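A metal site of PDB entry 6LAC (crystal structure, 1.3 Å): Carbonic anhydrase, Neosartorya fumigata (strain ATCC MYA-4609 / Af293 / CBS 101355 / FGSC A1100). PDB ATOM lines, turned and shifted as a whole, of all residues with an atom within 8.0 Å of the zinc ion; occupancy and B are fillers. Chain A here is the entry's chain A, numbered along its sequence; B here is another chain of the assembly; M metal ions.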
ATOM      1  N   GLY A  33      15.240  27.148  17.367  1.00  0.00           N
ATOM      2  CA  GLY A  33      16.268  27.141  18.406  1.00  0.00           C
ATOM      3  C   GLY A  33      16.215  25.816  19.145  1.00  0.00           C
ATOM      4  O   GLY A  33      15.375  24.927  18.917  1.00  0.00           O
ATOM      5  N   CYS A  34      17.146  25.677  20.064  1.00  0.00           N
ATOM      6  CA  CYS A  34      17.326  24.429  20.872  1.00  0.00           C
ATOM      7  C   CYS A  34      16.712  24.567  22.261  1.00  0.00           C
ATOM      8  O   CYS A  34      16.825  25.585  22.947  1.00  0.00           O
ATOM      9  CB  CYS A  34      18.787  24.085  21.014  1.00  0.00           C
ATOM     10  SG  CYS A  34      19.063  22.558  21.951  1.00  0.00           S
ATOM     11  N   SER A  35      16.048  23.495  22.669  1.00  0.00           N
ATOM     12  CA  SER A  35      15.412  23.400  24.001  1.00  0.00           C
ATOM     13  C   SER A  35      16.357  23.665  25.168  1.00  0.00           C
ATOM     14  O   SER A  35      15.831  24.132  26.199  1.00  0.00           O
ATOM     15  CB  SER A  35      14.794  22.053  24.141  1.00  0.00           C
ATOM     16  OG  SER A  35      13.769  21.851  23.163  1.00  0.00           O
ATOM     17  N   ASP A  36      17.654  23.369  25.071  1.00  0.00           N
ATOM     18  CA  ASP A  36      18.554  23.615  26.249  1.00  0.00           C
ATOM     19  C   ASP A  36      19.327  24.919  26.081  1.00  0.00           C
ATOM     20  O   ASP A  36      20.269  25.147  26.849  1.00  0.00           O
ATOM     21  CB  ASP A  36      19.436  22.414  26.588  1.00  0.00           C
ATOM     22  CG  ASP A  36      20.495  22.102  25.546  1.00  0.00           C
ATOM     23  OD1 ASP A  36      20.800  22.979  24.694  1.00  0.00           O
ATOM     24  OD2 ASP A  36      21.103  21.041  25.589  1.00  0.00           O
ATOM     25  N   SER A  37      18.904  25.859  25.237  1.00  0.00           N
ATOM     26  CA  SER A  37      19.674  27.112  25.052  1.00  0.00           C
ATOM     27  C   SER A  37      19.833  27.756  26.433  1.00  0.00           C
ATOM     28  O   SER A  37      20.918  28.251  26.746  1.00  0.00           O
ATOM     29  CB  SER A  37      19.026  27.950  24.030  1.00  0.00           C
ATOM     30  OG  SER A  37      19.769  29.135  23.793  1.00  0.00           O
ATOM     31  N   GLY A  38      18.780  27.856  27.231  1.00  0.00           N
ATOM     32  CA  GLY A  38      18.931  28.132  28.694  1.00  0.00           C
ATOM     33  C   GLY A  38      19.459  29.515  28.990  1.00  0.00           C
ATOM     34  O   GLY A  38      20.099  29.665  30.097  1.00  0.00           O
ATOM     35  N   GLU A  41      19.028  33.909  24.275  1.00  0.00           N
ATOM     36  CA  GLU A  41      19.230  33.819  22.817  1.00  0.00           C
ATOM     37  C   GLU A  41      18.378  34.795  22.015  1.00  0.00           C
ATOM     38  O   GLU A  41      18.910  35.445  21.115  1.00  0.00           O
ATOM     39  CB  GLU A  41      18.877  32.392  22.410  1.00  0.00           C
ATOM     40  CG  GLU A  41      18.935  32.103  20.934  1.00  0.00           C
ATOM     41  CD  GLU A  41      18.521  30.670  20.717  1.00  0.00           C
ATOM     42  OE1 GLU A  41      17.600  30.437  19.914  1.00  0.00           O
ATOM     43  OE2 GLU A  41      19.188  29.798  21.271  1.00  0.00           O
ATOM     44  N   ARG A  56      11.052  25.574  19.175  1.00  0.00           N
ATOM     45  CA  ARG A  56      12.232  25.248  20.017  1.00  0.00           C
ATOM     46  C   ARG A  56      12.214  23.779  20.306  1.00  0.00           C
ATOM     47  O   ARG A  56      11.264  23.286  20.914  1.00  0.00           O
ATOM     48  CB  ARG A  56      12.320  26.133  21.232  1.00  0.00           C
ATOM     49  CG  ARG A  56      13.642  25.949  21.959  1.00  0.00           C
ATOM     50  CD  ARG A  56      13.873  27.100  22.906  1.00  0.00           C
ATOM     51  NE  ARG A  56      14.048  28.402  22.257  1.00  0.00           N
ATOM     52  CZ  ARG A  56      15.174  28.908  21.766  1.00  0.00           C
ATOM     53  NH1 ARG A  56      16.305  28.250  21.832  1.00  0.00           N
ATOM     54  NH2 ARG A  56      15.119  30.082  21.153  1.00  0.00           N
ATOM     55  N   SER A  57      13.261  23.074  19.880  1.00  0.00           N
ATOM     56  CA  SER A  57      13.295  21.618  19.713  1.00  0.00           C
ATOM     57  C   SER A  57      14.608  21.048  20.146  1.00  0.00           C
ATOM     58  O   SER A  57      15.595  21.778  20.300  1.00  0.00           O
ATOM     59  CB  SER A  57      13.154  21.343  18.185  1.00  0.00           C
ATOM     60  OG  SER A  57      14.250  21.820  17.408  1.00  0.00           O
ATOM     61  N   LEU A  58      14.697  19.736  20.165  1.00  0.00           N
ATOM     62  CA  LEU A  58      15.976  19.075  20.486  1.00  0.00           C
ATOM     63  C   LEU A  58      17.026  19.455  19.462  1.00  0.00           C
ATOM     64  O   LEU A  58      16.855  19.178  18.271  1.00  0.00           O
ATOM     65  CB  LEU A  58      15.798  17.572  20.482  1.00  0.00           C
ATOM     66  CG  LEU A  58      14.842  16.971  21.519  1.00  0.00           C
ATOM     67  CD1 LEU A  58      14.636  15.499  21.244  1.00  0.00           C
ATOM     68  CD2 LEU A  58      15.394  17.209  22.924  1.00  0.00           C
ATOM     69  N   GLY A  59      18.120  20.010  19.913  1.00  0.00           N
ATOM     70  CA  GLY A  59      19.281  20.274  19.035  1.00  0.00           C
ATOM     71  C   GLY A  59      19.018  21.312  17.965  1.00  0.00           C
ATOM     72  O   GLY A  59      19.834  21.384  17.028  1.00  0.00           O
ATOM     73  N   ASN A  60      17.976  22.110  18.047  1.00  0.00           N
ATOM     74  CA  ASN A  60      17.599  23.073  16.979  1.00  0.00           C
ATOM     75  C   ASN A  60      17.600  22.339  15.652  1.00  0.00           C
ATOM     76  O   ASN A  60      18.100  22.860  14.624  1.00  0.00           O
ATOM     77  CB  ASN A  60      18.458  24.350  16.951  1.00  0.00           C
ATOM     78  CG  ASN A  60      19.945  24.164  17.022  1.00  0.00           C
ATOM     79  OD1 ASN A  60      20.520  24.150  18.117  1.00  0.00           O
ATOM     80  ND2 ASN A  60      20.623  24.124  15.867  1.00  0.00           N
ATOM     81  N   CYS A  87      19.030  28.726  14.739  1.00  0.00           N
ATOM     82  CA  CYS A  87      19.978  29.256  15.719  1.00  0.00           C
ATOM     83  C   CYS A  87      20.494  28.134  16.591  1.00  0.00           C
ATOM     84  O   CYS A  87      19.704  27.546  17.371  1.00  0.00           O
ATOM     85  CB  CYS A  87      19.332  30.287  16.581  1.00  0.00           C
ATOM     86  SG  CYS A  87      20.508  31.176  17.627  1.00  0.00           S
ATOM     87  N   GLY A  88      21.757  27.787  16.531  1.00  0.00           N
ATOM     88  CA  GLY A  88      22.421  26.930  17.517  1.00  0.00           C
ATOM     89  C   GLY A  88      23.005  27.740  18.619  1.00  0.00           C
ATOM     90  O   GLY A  88      22.894  28.981  18.635  1.00  0.00           O
ATOM     91  N   HIS A  89      23.586  27.044  19.600  1.00  0.00           N
ATOM     92  CA  HIS A  89      24.141  27.793  20.741  1.00  0.00           C
ATOM     93  C   HIS A  89      25.309  27.037  21.355  1.00  0.00           C
ATOM     94  O   HIS A  89      25.240  25.852  21.587  1.00  0.00           O
ATOM     95  CB  HIS A  89      23.026  28.107  21.773  1.00  0.00           C
ATOM     96  CG  HIS A  89      22.521  26.902  22.430  1.00  0.00           C
ATOM     97  ND1 HIS A  89      22.889  26.526  23.722  1.00  0.00           N
ATOM     98  CD2 HIS A  89      21.825  25.875  21.935  1.00  0.00           C
ATOM     99  CE1 HIS A  89      22.366  25.366  23.982  1.00  0.00           C
ATOM    100  NE2 HIS A  89      21.698  24.939  22.917  1.00  0.00           N
ATOM    101  N   TYR A  90      26.342  27.815  21.612  1.00  0.00           N
ATOM    102  CA  TYR A  90      27.502  27.232  22.322  1.00  0.00           C
ATOM    103  C   TYR A  90      27.105  26.732  23.714  1.00  0.00           C
ATOM    104  O   TYR A  90      26.365  27.409  24.414  1.00  0.00           O
ATOM    105  CB  TYR A  90      28.673  28.190  22.324  1.00  0.00           C
ATOM    106  CG  TYR A  90      29.160  28.588  20.943  1.00  0.00           C
ATOM    107  CD1 TYR A  90      29.660  27.648  20.048  1.00  0.00           C
ATOM    108  CD2 TYR A  90      29.180  29.903  20.553  1.00  0.00           C
ATOM    109  CE1 TYR A  90      30.082  28.009  18.776  1.00  0.00           C
ATOM    110  CE2 TYR A  90      29.608  30.292  19.292  1.00  0.00           C
ATOM    111  CZ  TYR A  90      30.087  29.342  18.421  1.00  0.00           C
ATOM    112  OH  TYR A  90      30.530  29.791  17.194  1.00  0.00           O
ATOM    113  N   GLY A  91      27.668  25.591  24.074  1.00  0.00           N
ATOM    114  CA  GLY A  91      27.381  24.929  25.350  1.00  0.00           C
ATOM    115  C   GLY A  91      26.246  23.946  25.279  1.00  0.00           C
ATOM    116  O   GLY A  91      25.871  23.362  26.310  1.00  0.00           O
ATOM    117  N   CYS A  92      25.605  23.801  24.123  1.00  0.00           N
ATOM    118  CA  CYS A  92      24.546  22.801  23.876  1.00  0.00           C
ATOM    119  C   CYS A  92      24.943  21.448  24.456  1.00  0.00           C
ATOM    120  O   CYS A  92      26.018  20.971  24.197  1.00  0.00           O
ATOM    121  CB  CYS A  92      24.354  22.709  22.380  1.00  0.00           C
ATOM    122  SG  CYS A  92      22.881  21.765  21.897  1.00  0.00           S
ATOM    123  N   HIS A  93      24.066  20.794  25.206  1.00  0.00           N
ATOM    124  CA  HIS A  93      24.296  19.442  25.731  1.00  0.00           C
ATOM    125  C   HIS A  93      23.858  18.419  24.719  1.00  0.00           C
ATOM    126  O   HIS A  93      24.320  17.257  24.713  1.00  0.00           O
ATOM    127  CB  HIS A  93      23.612  19.233  27.090  1.00  0.00           C
ATOM    128  CG  HIS A  93      24.136  20.145  28.126  1.00  0.00           C
ATOM    129  ND1 HIS A  93      25.286  19.899  28.842  1.00  0.00           N
ATOM    130  CD2 HIS A  93      23.698  21.344  28.541  1.00  0.00           C
ATOM    131  CE1 HIS A  93      25.508  20.918  29.665  1.00  0.00           C
ATOM    132  NE2 HIS A  93      24.558  21.807  29.492  1.00  0.00           N
ATOM    133  N   ILE A  94      23.012  18.788  23.763  1.00  0.00           N
ATOM    134  CA  ILE A  94      22.514  17.830  22.763  1.00  0.00           C
ATOM    135  C   ILE A  94      23.549  17.737  21.645  1.00  0.00           C
ATOM    136  O   ILE A  94      23.987  16.586  21.305  1.00  0.00           O
ATOM    137  CB  ILE A  94      21.081  18.236  22.332  1.00  0.00           C
ATOM    138  CG1 ILE A  94      20.100  18.098  23.499  1.00  0.00           C
ATOM    139  CG2 ILE A  94      20.654  17.427  21.136  1.00  0.00           C
ATOM    140  CD1 ILE A  94      18.811  18.811  23.244  1.00  0.00           C
ATOM    141  N   ALA A  95      23.939  18.823  20.986  1.00  0.00           N
ATOM    142  CA  ALA A  95      24.992  18.795  19.916  1.00  0.00           C
ATOM    143  C   ALA A  95      26.362  18.907  20.574  1.00  0.00           C
ATOM    144  O   ALA A  95      26.961  19.967  20.602  1.00  0.00           O
ATOM    145  CB  ALA A  95      24.741  19.842  18.863  1.00  0.00           C
ATOM    146  N   SER A  96      26.775  17.812  21.225  1.00  0.00           N
ATOM    147  CA  SER A  96      28.006  17.799  22.045  1.00  0.00           C
ATOM    148  C   SER A  96      28.485  16.369  22.168  1.00  0.00           C
ATOM    149  O   SER A  96      27.709  15.433  21.975  1.00  0.00           O
ATOM    150  CB  SER A  96      27.852  18.436  23.403  1.00  0.00           C
ATOM    151  OG  SER A  96      27.474  17.515  24.407  1.00  0.00           O
ATOM    152  N   VAL A 135      28.419  22.217  17.259  1.00  0.00           N
ATOM    153  CA  VAL A 135      27.246  23.151  17.239  1.00  0.00           C
ATOM    154  C   VAL A 135      27.148  23.828  15.869  1.00  0.00           C
ATOM    155  O   VAL A 135      26.064  23.954  15.296  1.00  0.00           O
ATOM    156  CB  VAL A 135      27.355  24.150  18.386  1.00  0.00           C
ATOM    157  CG1 VAL A 135      26.449  25.332  18.201  1.00  0.00           C
ATOM    158  CG2 VAL A 135      27.064  23.485  19.719  1.00  0.00           C
ATOM    159  N   ASN A 138      26.234  21.471  12.988  1.00  0.00           N
ATOM    160  CA  ASN A 138      24.805  21.098  13.060  1.00  0.00           C
ATOM    161  C   ASN A 138      23.969  22.229  12.442  1.00  0.00           C
ATOM    162  O   ASN A 138      23.040  21.939  11.703  1.00  0.00           O
ATOM    163  CB  ASN A 138      24.420  20.753  14.481  1.00  0.00           C
ATOM    164  CG  ASN A 138      23.004  20.314  14.631  1.00  0.00           C
ATOM    165  OD1 ASN A 138      22.584  19.402  13.930  1.00  0.00           O
ATOM    166  ND2 ASN A 138      22.290  20.974  15.551  1.00  0.00           N
ATOM    167  N   PHE B  53      13.984  24.038  30.260  1.00  0.00           N
ATOM    168  CA  PHE B  53      14.207  23.167  29.091  1.00  0.00           C
ATOM    169  C   PHE B  53      12.942  23.335  28.271  1.00  0.00           C
ATOM    170  O   PHE B  53      11.882  22.894  28.673  1.00  0.00           O
ATOM    171  CB  PHE B  53      14.466  21.733  29.541  1.00  0.00           C
ATOM    172  CG  PHE B  53      14.764  20.827  28.399  1.00  0.00           C
ATOM    173  CD1 PHE B  53      16.005  20.844  27.790  1.00  0.00           C
ATOM    174  CD2 PHE B  53      13.833  19.936  27.952  1.00  0.00           C
ATOM    175  CE1 PHE B  53      16.279  20.003  26.729  1.00  0.00           C
ATOM    176  CE2 PHE B  53      14.086  19.106  26.876  1.00  0.00           C
ATOM    177  CZ  PHE B  53      15.331  19.126  26.304  1.00  0.00           C
ATOM    178  N   TYR B  74      13.787  12.374  26.430  1.00  0.00           N
ATOM    179  CA  TYR B  74      15.068  12.995  26.794  1.00  0.00           C
ATOM    180  C   TYR B  74      14.937  13.731  28.136  1.00  0.00           C
ATOM    181  O   TYR B  74      15.809  13.655  28.998  1.00  0.00           O
ATOM    182  CB  TYR B  74      15.548  13.937  25.670  1.00  0.00           C
ATOM    183  CG  TYR B  74      16.831  14.652  25.924  1.00  0.00           C
ATOM    184  CD1 TYR B  74      18.032  14.023  25.697  1.00  0.00           C
ATOM    185  CD2 TYR B  74      16.881  15.930  26.433  1.00  0.00           C
ATOM    186  CE1 TYR B  74      19.228  14.666  25.969  1.00  0.00           C
ATOM    187  CE2 TYR B  74      18.064  16.588  26.695  1.00  0.00           C
ATOM    188  CZ  TYR B  74      19.264  15.945  26.458  1.00  0.00           C
ATOM    189  OH  TYR B  74      20.400  16.606  26.738  1.00  0.00           O
HETATM  190 ZN    ZN M   1      21.111  22.961  22.782  1.00  0.00          ZN
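N of His 93 lies within hydrogen-bond range of OD2 of Asp 36. OD2 of Asp 36 sits at hydrogen-bond distance from N of Ile 94. SG of Cys 34 sits close to N of Gly 59, 3.4 Å away. NH1 of Arg 56 is in hydrogen-bond range of O of Cys 34, 2.9 Å away. N of Ile 94 sits close to SG of Cys 92, 3.5 Å away. SG of Cys 92 lies close to N of Ala 95 (3.3 Å).
Within 4 Å of the zinc ion: Cys 34, Asp 36, His 89 and Cys 92.
The zinc ion is bound by OD1 of Asp 36 (1.9 Å), NE2 of His 89 (2.1 Å), SG of Cys 34 (2.2 Å) and SG of Cys 92 (2.3 Å). The zinc ion has four donor atoms within binding distance.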
